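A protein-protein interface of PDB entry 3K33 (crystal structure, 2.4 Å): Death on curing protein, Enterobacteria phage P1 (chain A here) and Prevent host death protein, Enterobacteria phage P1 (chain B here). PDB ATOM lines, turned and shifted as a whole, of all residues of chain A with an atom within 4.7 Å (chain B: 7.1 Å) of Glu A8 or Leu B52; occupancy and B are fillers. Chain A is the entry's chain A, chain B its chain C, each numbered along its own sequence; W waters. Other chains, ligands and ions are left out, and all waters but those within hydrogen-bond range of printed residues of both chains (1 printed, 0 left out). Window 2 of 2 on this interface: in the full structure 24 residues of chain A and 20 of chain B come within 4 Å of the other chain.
Printed residues of chain B within 4 Å of Glu A8: Leu B52 (3.8 Å) and Phe B56 (3.7 Å).
Leu B52 touches two residues of chain A.
Of the printed residues of chain B, Leu A12 touches Phe B56.
Printed residues of chain A within 4 Å of Phe B56: Glu A8 (3.7 Å), Ala A11 (3.5 Å) and Leu A12 (3.5 Å).
Printed residues of chain A within 4 Å of Glu B55: Arg A86 (2.8 Å).
Printed residues of chain B within 4 Å of Arg A86: Leu B52 and Glu B55.
Ile A4 touches none of the printed residues of chain B.
The nearest printed residue of chain A that does not touch Leu B52 is Ala A11 (4.9 Å).
The nearest printed residue of chain B that does not touch Leu A12 is Leu B52 (7.0 Å).
The backbone carbonyl oxygen (O) of His A3 lies within hydrogen-bond range of the guanidinium group (NH1) of Arg A86 (2.9 Å).
The backbone NH (N) of Ser A5 lies within hydrogen-bond range of the side-chain carboxylate (OE1) of Glu A8.
The side-chain carboxylate of Glu A8 lies within salt-bridge range of the guanidinium group of Arg A86.
OG of Ser B58 sits at hydrogen-bond distance from O of Glu B55 (3.5 Å).
OE1 of Glu A7 is in salt-bridge range of NZ of Lys B48, 3.5 Å away.
NH2 of Arg A86 is in salt-bridge range of OE1 of Glu B55, 2.8 Å away.
Of the 12 printed residues of chain B, 4 touch a printed residue of chain A.
Hydrophobic or aromatic side chains of chain B within 4 Å of the printed part of chain A: Leu B52 and Phe B56.
Hydrophobic or aromatic side chains of chain A that line the printed part of chain B: Ala A11 and Leu A12.
Among the printed residues, pairs that only touch across the chains: Glu A8 with Leu B52 (3.8 Å), Glu A8 with Phe B56 (3.7 Å), Ala A11 with Phe B56 (3.5 Å), Leu A12 with Phe B56 (3.5 Å) and Arg A86 with Leu B52 (3.9 Å).
Water W1 lies within hydrogen-bond range of OE1 of Glu A7 (3.1 Å) and NZ of Lys B48 (3.2 Å).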
ATOM      1  N   HIS A   3     -14.038   5.583 -26.039  1.00  0.00           N
ATOM      2  CA  HIS A   3     -14.532   5.281 -24.714  1.00  0.00           C
ATOM      3  C   HIS A   3     -13.566   4.388 -23.946  1.00  0.00           C
ATOM      4  O   HIS A   3     -12.552   3.931 -24.489  1.00  0.00           O
ATOM      5  CB  HIS A   3     -15.909   4.622 -24.815  1.00  0.00           C
ATOM      6  CG  HIS A   3     -17.022   5.586 -25.094  1.00  0.00           C
ATOM      7  ND1 HIS A   3     -17.563   6.400 -24.118  1.00  0.00           N
ATOM      8  CD2 HIS A   3     -17.702   5.860 -26.230  1.00  0.00           C
ATOM      9  CE1 HIS A   3     -18.530   7.130 -24.642  1.00  0.00           C
ATOM     10  NE2 HIS A   3     -18.632   6.824 -25.925  1.00  0.00           N
ATOM     11  N   ILE A   4     -13.873   4.173 -22.669  1.00  0.00           N
ATOM     12  CA  ILE A   4     -13.102   3.257 -21.835  1.00  0.00           C
ATOM     13  C   ILE A   4     -14.027   2.054 -21.702  1.00  0.00           C
ATOM     14  O   ILE A   4     -15.194   2.201 -21.339  1.00  0.00           O
ATOM     15  CB  ILE A   4     -12.802   3.828 -20.410  1.00  0.00           C
ATOM     16  CG1 ILE A   4     -12.378   5.314 -20.458  1.00  0.00           C
ATOM     17  CG2 ILE A   4     -11.759   2.957 -19.694  1.00  0.00           C
ATOM     18  CD1 ILE A   4     -11.295   5.649 -21.414  1.00  0.00           C
ATOM     19  N   SER A   5     -13.521   0.869 -22.018  1.00  0.00           N
ATOM     20  CA  SER A   5     -14.328  -0.324 -21.883  1.00  0.00           C
ATOM     21  C   SER A   5     -14.245  -0.815 -20.438  1.00  0.00           C
ATOM     22  O   SER A   5     -13.285  -0.514 -19.716  1.00  0.00           O
ATOM     23  CB  SER A   5     -13.850  -1.418 -22.850  1.00  0.00           C
ATOM     24  OG  SER A   5     -12.619  -1.947 -22.413  1.00  0.00           O
ATOM     25  N   PRO A   6     -15.263  -1.568 -20.000  1.00  0.00           N
ATOM     26  CA  PRO A   6     -15.276  -2.135 -18.661  1.00  0.00           C
ATOM     27  C   PRO A   6     -13.958  -2.852 -18.371  1.00  0.00           C
ATOM     28  O   PRO A   6     -13.394  -2.722 -17.285  1.00  0.00           O
ATOM     29  CB  PRO A   6     -16.454  -3.116 -18.731  1.00  0.00           C
ATOM     30  CG  PRO A   6     -17.417  -2.386 -19.633  1.00  0.00           C
ATOM     31  CD  PRO A   6     -16.488  -1.936 -20.744  1.00  0.00           C
ATOM     32  N   GLU A   7     -13.476  -3.590 -19.360  1.00  0.00           N
ATOM     33  CA  GLU A   7     -12.240  -4.354 -19.246  1.00  0.00           C
ATOM     34  C   GLU A   7     -11.011  -3.460 -19.078  1.00  0.00           C
ATOM     35  O   GLU A   7     -10.077  -3.804 -18.361  1.00  0.00           O
ATOM     36  CB  GLU A   7     -12.084  -5.256 -20.469  1.00  0.00           C
ATOM     37  CG  GLU A   7     -10.924  -6.206 -20.366  1.00  0.00           C
ATOM     38  CD  GLU A   7     -10.736  -7.065 -21.603  1.00  0.00           C
ATOM     39  OE1 GLU A   7      -9.773  -7.865 -21.607  1.00  0.00           O
ATOM     40  OE2 GLU A   7     -11.538  -6.947 -22.562  1.00  0.00           O
ATOM     41  N   GLU A   8     -11.015  -2.317 -19.751  1.00  0.00           N
ATOM     42  CA  GLU A   8      -9.943  -1.332 -19.596  1.00  0.00           C
ATOM     43  C   GLU A   8     -10.008  -0.673 -18.222  1.00  0.00           C
ATOM     44  O   GLU A   8      -8.977  -0.300 -17.665  1.00  0.00           O
ATOM     45  CB  GLU A   8     -10.025  -0.268 -20.699  1.00  0.00           C
ATOM     46  CG  GLU A   8      -9.841  -0.859 -22.099  1.00  0.00           C
ATOM     47  CD  GLU A   8      -9.792   0.185 -23.193  1.00  0.00           C
ATOM     48  OE1 GLU A   8     -10.700   1.039 -23.259  1.00  0.00           O
ATOM     49  OE2 GLU A   8      -8.849   0.130 -24.006  1.00  0.00           O
ATOM     50  N   LEU A   9     -11.213  -0.525 -17.675  1.00  0.00           N
ATOM     51  CA  LEU A   9     -11.361   0.068 -16.345  1.00  0.00           C
ATOM     52  C   LEU A   9     -10.764  -0.879 -15.311  1.00  0.00           C
ATOM     53  O   LEU A   9     -10.045  -0.458 -14.400  1.00  0.00           O
ATOM     54  CB  LEU A   9     -12.831   0.324 -16.007  1.00  0.00           C
ATOM     55  CG  LEU A   9     -12.996   1.225 -14.774  1.00  0.00           C
ATOM     56  CD1 LEU A   9     -12.949   2.679 -15.224  1.00  0.00           C
ATOM     57  CD2 LEU A   9     -14.290   0.935 -14.044  1.00  0.00           C
ATOM     58  N   ILE A  10     -11.060  -2.164 -15.463  1.00  0.00           N
ATOM     59  CA  ILE A  10     -10.508  -3.181 -14.571  1.00  0.00           C
ATOM     60  C   ILE A  10      -8.994  -3.121 -14.596  1.00  0.00           C
ATOM     61  O   ILE A  10      -8.350  -3.126 -13.546  1.00  0.00           O
ATOM     62  CB  ILE A  10     -10.947  -4.607 -14.986  1.00  0.00           C
ATOM     63  CG1 ILE A  10     -12.472  -4.731 -14.952  1.00  0.00           C
ATOM     64  CG2 ILE A  10     -10.295  -5.641 -14.079  1.00  0.00           C
ATOM     65  CD1 ILE A  10     -13.000  -6.086 -15.459  1.00  0.00           C
ATOM     66  N   ALA A  11      -8.434  -3.063 -15.803  1.00  0.00           N
ATOM     67  CA  ALA A  11      -6.990  -3.015 -15.987  1.00  0.00           C
ATOM     68  C   ALA A  11      -6.371  -1.713 -15.459  1.00  0.00           C
ATOM     69  O   ALA A  11      -5.299  -1.725 -14.849  1.00  0.00           O
ATOM     70  CB  ALA A  11      -6.645  -3.229 -17.458  1.00  0.00           C
ATOM     71  N   LEU A  12      -7.048  -0.593 -15.691  1.00  0.00           N
ATOM     72  CA  LEU A  12      -6.581   0.701 -15.195  1.00  0.00           C
ATOM     73  C   LEU A  12      -6.518   0.658 -13.666  1.00  0.00           C
ATOM     74  O   LEU A  12      -5.610   1.215 -13.050  1.00  0.00           O
ATOM     75  CB  LEU A  12      -7.533   1.808 -15.661  1.00  0.00           C
ATOM     76  CG  LEU A  12      -7.192   3.288 -15.464  1.00  0.00           C
ATOM     77  CD1 LEU A  12      -8.295   4.107 -16.104  1.00  0.00           C
ATOM     78  CD2 LEU A  12      -7.051   3.657 -13.993  1.00  0.00           C
ATOM     79  N   ARG A  86      -7.538  10.530 -24.490  1.00  0.00           N
ATOM     80  CA  ARG A  86      -7.861   9.657 -25.621  1.00  0.00           C
ATOM     81  C   ARG A  86      -8.692  10.350 -26.687  1.00  0.00           C
ATOM     82  O   ARG A  86      -8.759   9.875 -27.818  1.00  0.00           O
ATOM     83  CB  ARG A  86      -8.637   8.422 -25.158  1.00  0.00           C
ATOM     84  CG  ARG A  86      -7.798   7.295 -24.620  1.00  0.00           C
ATOM     85  CD  ARG A  86      -8.703   6.107 -24.346  1.00  0.00           C
ATOM     86  NE  ARG A  86      -7.924   4.927 -23.992  1.00  0.00           N
ATOM     87  CZ  ARG A  86      -8.425   3.706 -23.830  1.00  0.00           C
ATOM     88  NH1 ARG A  86      -9.724   3.477 -23.998  1.00  0.00           N
ATOM     89  NH2 ARG A  86      -7.615   2.710 -23.491  1.00  0.00           N
ATOM     90  N   TYR B  47       0.871  -7.995 -26.437  1.00  0.00           N
ATOM     91  CA  TYR B  47       0.894  -6.703 -27.124  1.00  0.00           C
ATOM     92  C   TYR B  47      -0.067  -5.721 -26.446  1.00  0.00           C
ATOM     93  O   TYR B  47       0.306  -4.588 -26.118  1.00  0.00           O
ATOM     94  CB  TYR B  47       0.521  -6.879 -28.602  1.00  0.00           C
ATOM     95  N   LYS B  48      -1.303  -6.140 -26.192  1.00  0.00           N
ATOM     96  CA  LYS B  48      -2.262  -5.230 -25.586  1.00  0.00           C
ATOM     97  C   LYS B  48      -1.967  -4.967 -24.128  1.00  0.00           C
ATOM     98  O   LYS B  48      -2.213  -3.884 -23.649  1.00  0.00           O
ATOM     99  CB  LYS B  48      -3.707  -5.671 -25.840  1.00  0.00           C
ATOM    100  CG  LYS B  48      -4.483  -6.212 -24.675  1.00  0.00           C
ATOM    101  CD  LYS B  48      -5.855  -5.629 -24.694  1.00  0.00           C
ATOM    102  CE  LYS B  48      -6.893  -6.620 -24.314  1.00  0.00           C
ATOM    103  NZ  LYS B  48      -8.151  -5.925 -24.055  1.00  0.00           N
ATOM    104  N   LYS B  49      -1.416  -5.950 -23.430  1.00  0.00           N
ATOM    105  CA  LYS B  49      -0.945  -5.678 -22.073  1.00  0.00           C
ATOM    106  C   LYS B  49       0.196  -4.664 -22.135  1.00  0.00           C
ATOM    107  O   LYS B  49       0.261  -3.737 -21.321  1.00  0.00           O
ATOM    108  CB  LYS B  49      -0.476  -6.971 -21.389  1.00  0.00           C
ATOM    109  N   ALA B  50       1.081  -4.839 -23.115  1.00  0.00           N
ATOM    110  CA  ALA B  50       2.197  -3.918 -23.324  1.00  0.00           C
ATOM    111  C   ALA B  50       1.714  -2.480 -23.549  1.00  0.00           C
ATOM    112  O   ALA B  50       2.165  -1.559 -22.871  1.00  0.00           O
ATOM    113  N   ALA B  51       0.786  -2.305 -24.493  1.00  0.00           N
ATOM    114  CA  ALA B  51       0.266  -0.990 -24.852  1.00  0.00           C
ATOM    115  C   ALA B  51      -0.462  -0.273 -23.705  1.00  0.00           C
ATOM    116  O   ALA B  51      -0.158   0.887 -23.409  1.00  0.00           O
ATOM    117  CB  ALA B  51      -0.648  -1.102 -26.071  1.00  0.00           C
ATOM    118  N   LEU B  52      -1.408  -0.964 -23.067  1.00  0.00           N
ATOM    119  CA  LEU B  52      -2.199  -0.384 -21.977  1.00  0.00           C
ATOM    120  C   LEU B  52      -1.340  -0.081 -20.760  1.00  0.00           C
ATOM    121  O   LEU B  52      -1.542   0.931 -20.100  1.00  0.00           O
ATOM    122  CB  LEU B  52      -3.354  -1.316 -21.579  1.00  0.00           C
ATOM    123  CG  LEU B  52      -4.451  -1.585 -22.624  1.00  0.00           C
ATOM    124  CD1 LEU B  52      -5.328  -2.745 -22.188  1.00  0.00           C
ATOM    125  CD2 LEU B  52      -5.291  -0.336 -22.866  1.00  0.00           C
ATOM    126  N   ASP B  53      -0.381  -0.952 -20.460  1.00  0.00           N
ATOM    127  CA  ASP B  53       0.530  -0.694 -19.342  1.00  0.00           C
ATOM    128  C   ASP B  53       1.227   0.645 -19.505  1.00  0.00           C
ATOM    129  O   ASP B  53       1.412   1.380 -18.530  1.00  0.00           O
ATOM    130  CB  ASP B  53       1.587  -1.797 -19.216  1.00  0.00           C
ATOM    131  CG  ASP B  53       1.057  -3.034 -18.522  1.00  0.00           C
ATOM    132  OD1 ASP B  53       1.825  -4.008 -18.396  1.00  0.00           O
ATOM    133  OD2 ASP B  53      -0.116  -3.028 -18.087  1.00  0.00           O
ATOM    134  N   ALA B  54       1.610   0.952 -20.740  1.00  0.00           N
ATOM    135  CA  ALA B  54       2.324   2.187 -21.037  1.00  0.00           C
ATOM    136  C   ALA B  54       1.384   3.381 -21.054  1.00  0.00           C
ATOM    137  O   ALA B  54       1.754   4.471 -20.611  1.00  0.00           O
ATOM    138  CB  ALA B  54       3.069   2.065 -22.373  1.00  0.00           C
ATOM    139  N   GLU B  55       0.173   3.168 -21.577  1.00  0.00           N
ATOM    140  CA  GLU B  55      -0.844   4.212 -21.629  1.00  0.00           C
ATOM    141  C   GLU B  55      -1.274   4.593 -20.212  1.00  0.00           C
ATOM    142  O   GLU B  55      -1.508   5.763 -19.935  1.00  0.00           O
ATOM    143  CB  GLU B  55      -2.061   3.767 -22.465  1.00  0.00           C
ATOM    144  CG  GLU B  55      -3.229   4.764 -22.431  1.00  0.00           C
ATOM    145  CD  GLU B  55      -4.413   4.382 -23.312  1.00  0.00           C
ATOM    146  OE1 GLU B  55      -4.828   3.203 -23.309  1.00  0.00           O
ATOM    147  OE2 GLU B  55      -4.959   5.281 -23.987  1.00  0.00           O
ATOM    148  N   PHE B  56      -1.369   3.611 -19.319  1.00  0.00           N
ATOM    149  CA  PHE B  56      -1.729   3.876 -17.924  1.00  0.00           C
ATOM    150  C   PHE B  56      -0.536   4.440 -17.168  1.00  0.00           C
ATOM    151  O   PHE B  56      -0.669   5.411 -16.429  1.00  0.00           O
ATOM    152  CB  PHE B  56      -2.162   2.605 -17.183  1.00  0.00           C
ATOM    153  CG  PHE B  56      -3.326   1.875 -17.802  1.00  0.00           C
ATOM    154  CD1 PHE B  56      -4.308   2.548 -18.507  1.00  0.00           C
ATOM    155  CD2 PHE B  56      -3.471   0.507 -17.591  1.00  0.00           C
ATOM    156  CE1 PHE B  56      -5.396   1.881 -19.018  1.00  0.00           C
ATOM    157  CE2 PHE B  56      -4.566  -0.170 -18.091  1.00  0.00           C
ATOM    158  CZ  PHE B  56      -5.535   0.521 -18.799  1.00  0.00           C
ATOM    159  N   ALA B  57       0.618   3.792 -17.338  1.00  0.00           N
ATOM    160  CA  ALA B  57       1.856   4.164 -16.643  1.00  0.00           C
ATOM    161  C   ALA B  57       2.173   5.644 -16.729  1.00  0.00           C
ATOM    162  O   ALA B  57       2.619   6.240 -15.748  1.00  0.00           O
ATOM    163  CB  ALA B  57       3.036   3.356 -17.181  1.00  0.00           C
ATOM    164  N   SER B  58       1.959   6.221 -17.906  1.00  0.00           N
ATOM    165  CA  SER B  58       2.229   7.630 -18.133  1.00  0.00           C
ATOM    166  C   SER B  58       1.075   8.468 -17.623  1.00  0.00           C
ATOM    167  O   SER B  58       1.260   9.632 -17.266  1.00  0.00           O
ATOM    168  CB  SER B  58       2.461   7.906 -19.622  1.00  0.00           C
ATOM    169  OG  SER B  58       1.269   7.772 -20.370  1.00  0.00           O
HETATM  170  O   HOH W   1      -7.693  -5.648 -20.883  1.00  0.00           O
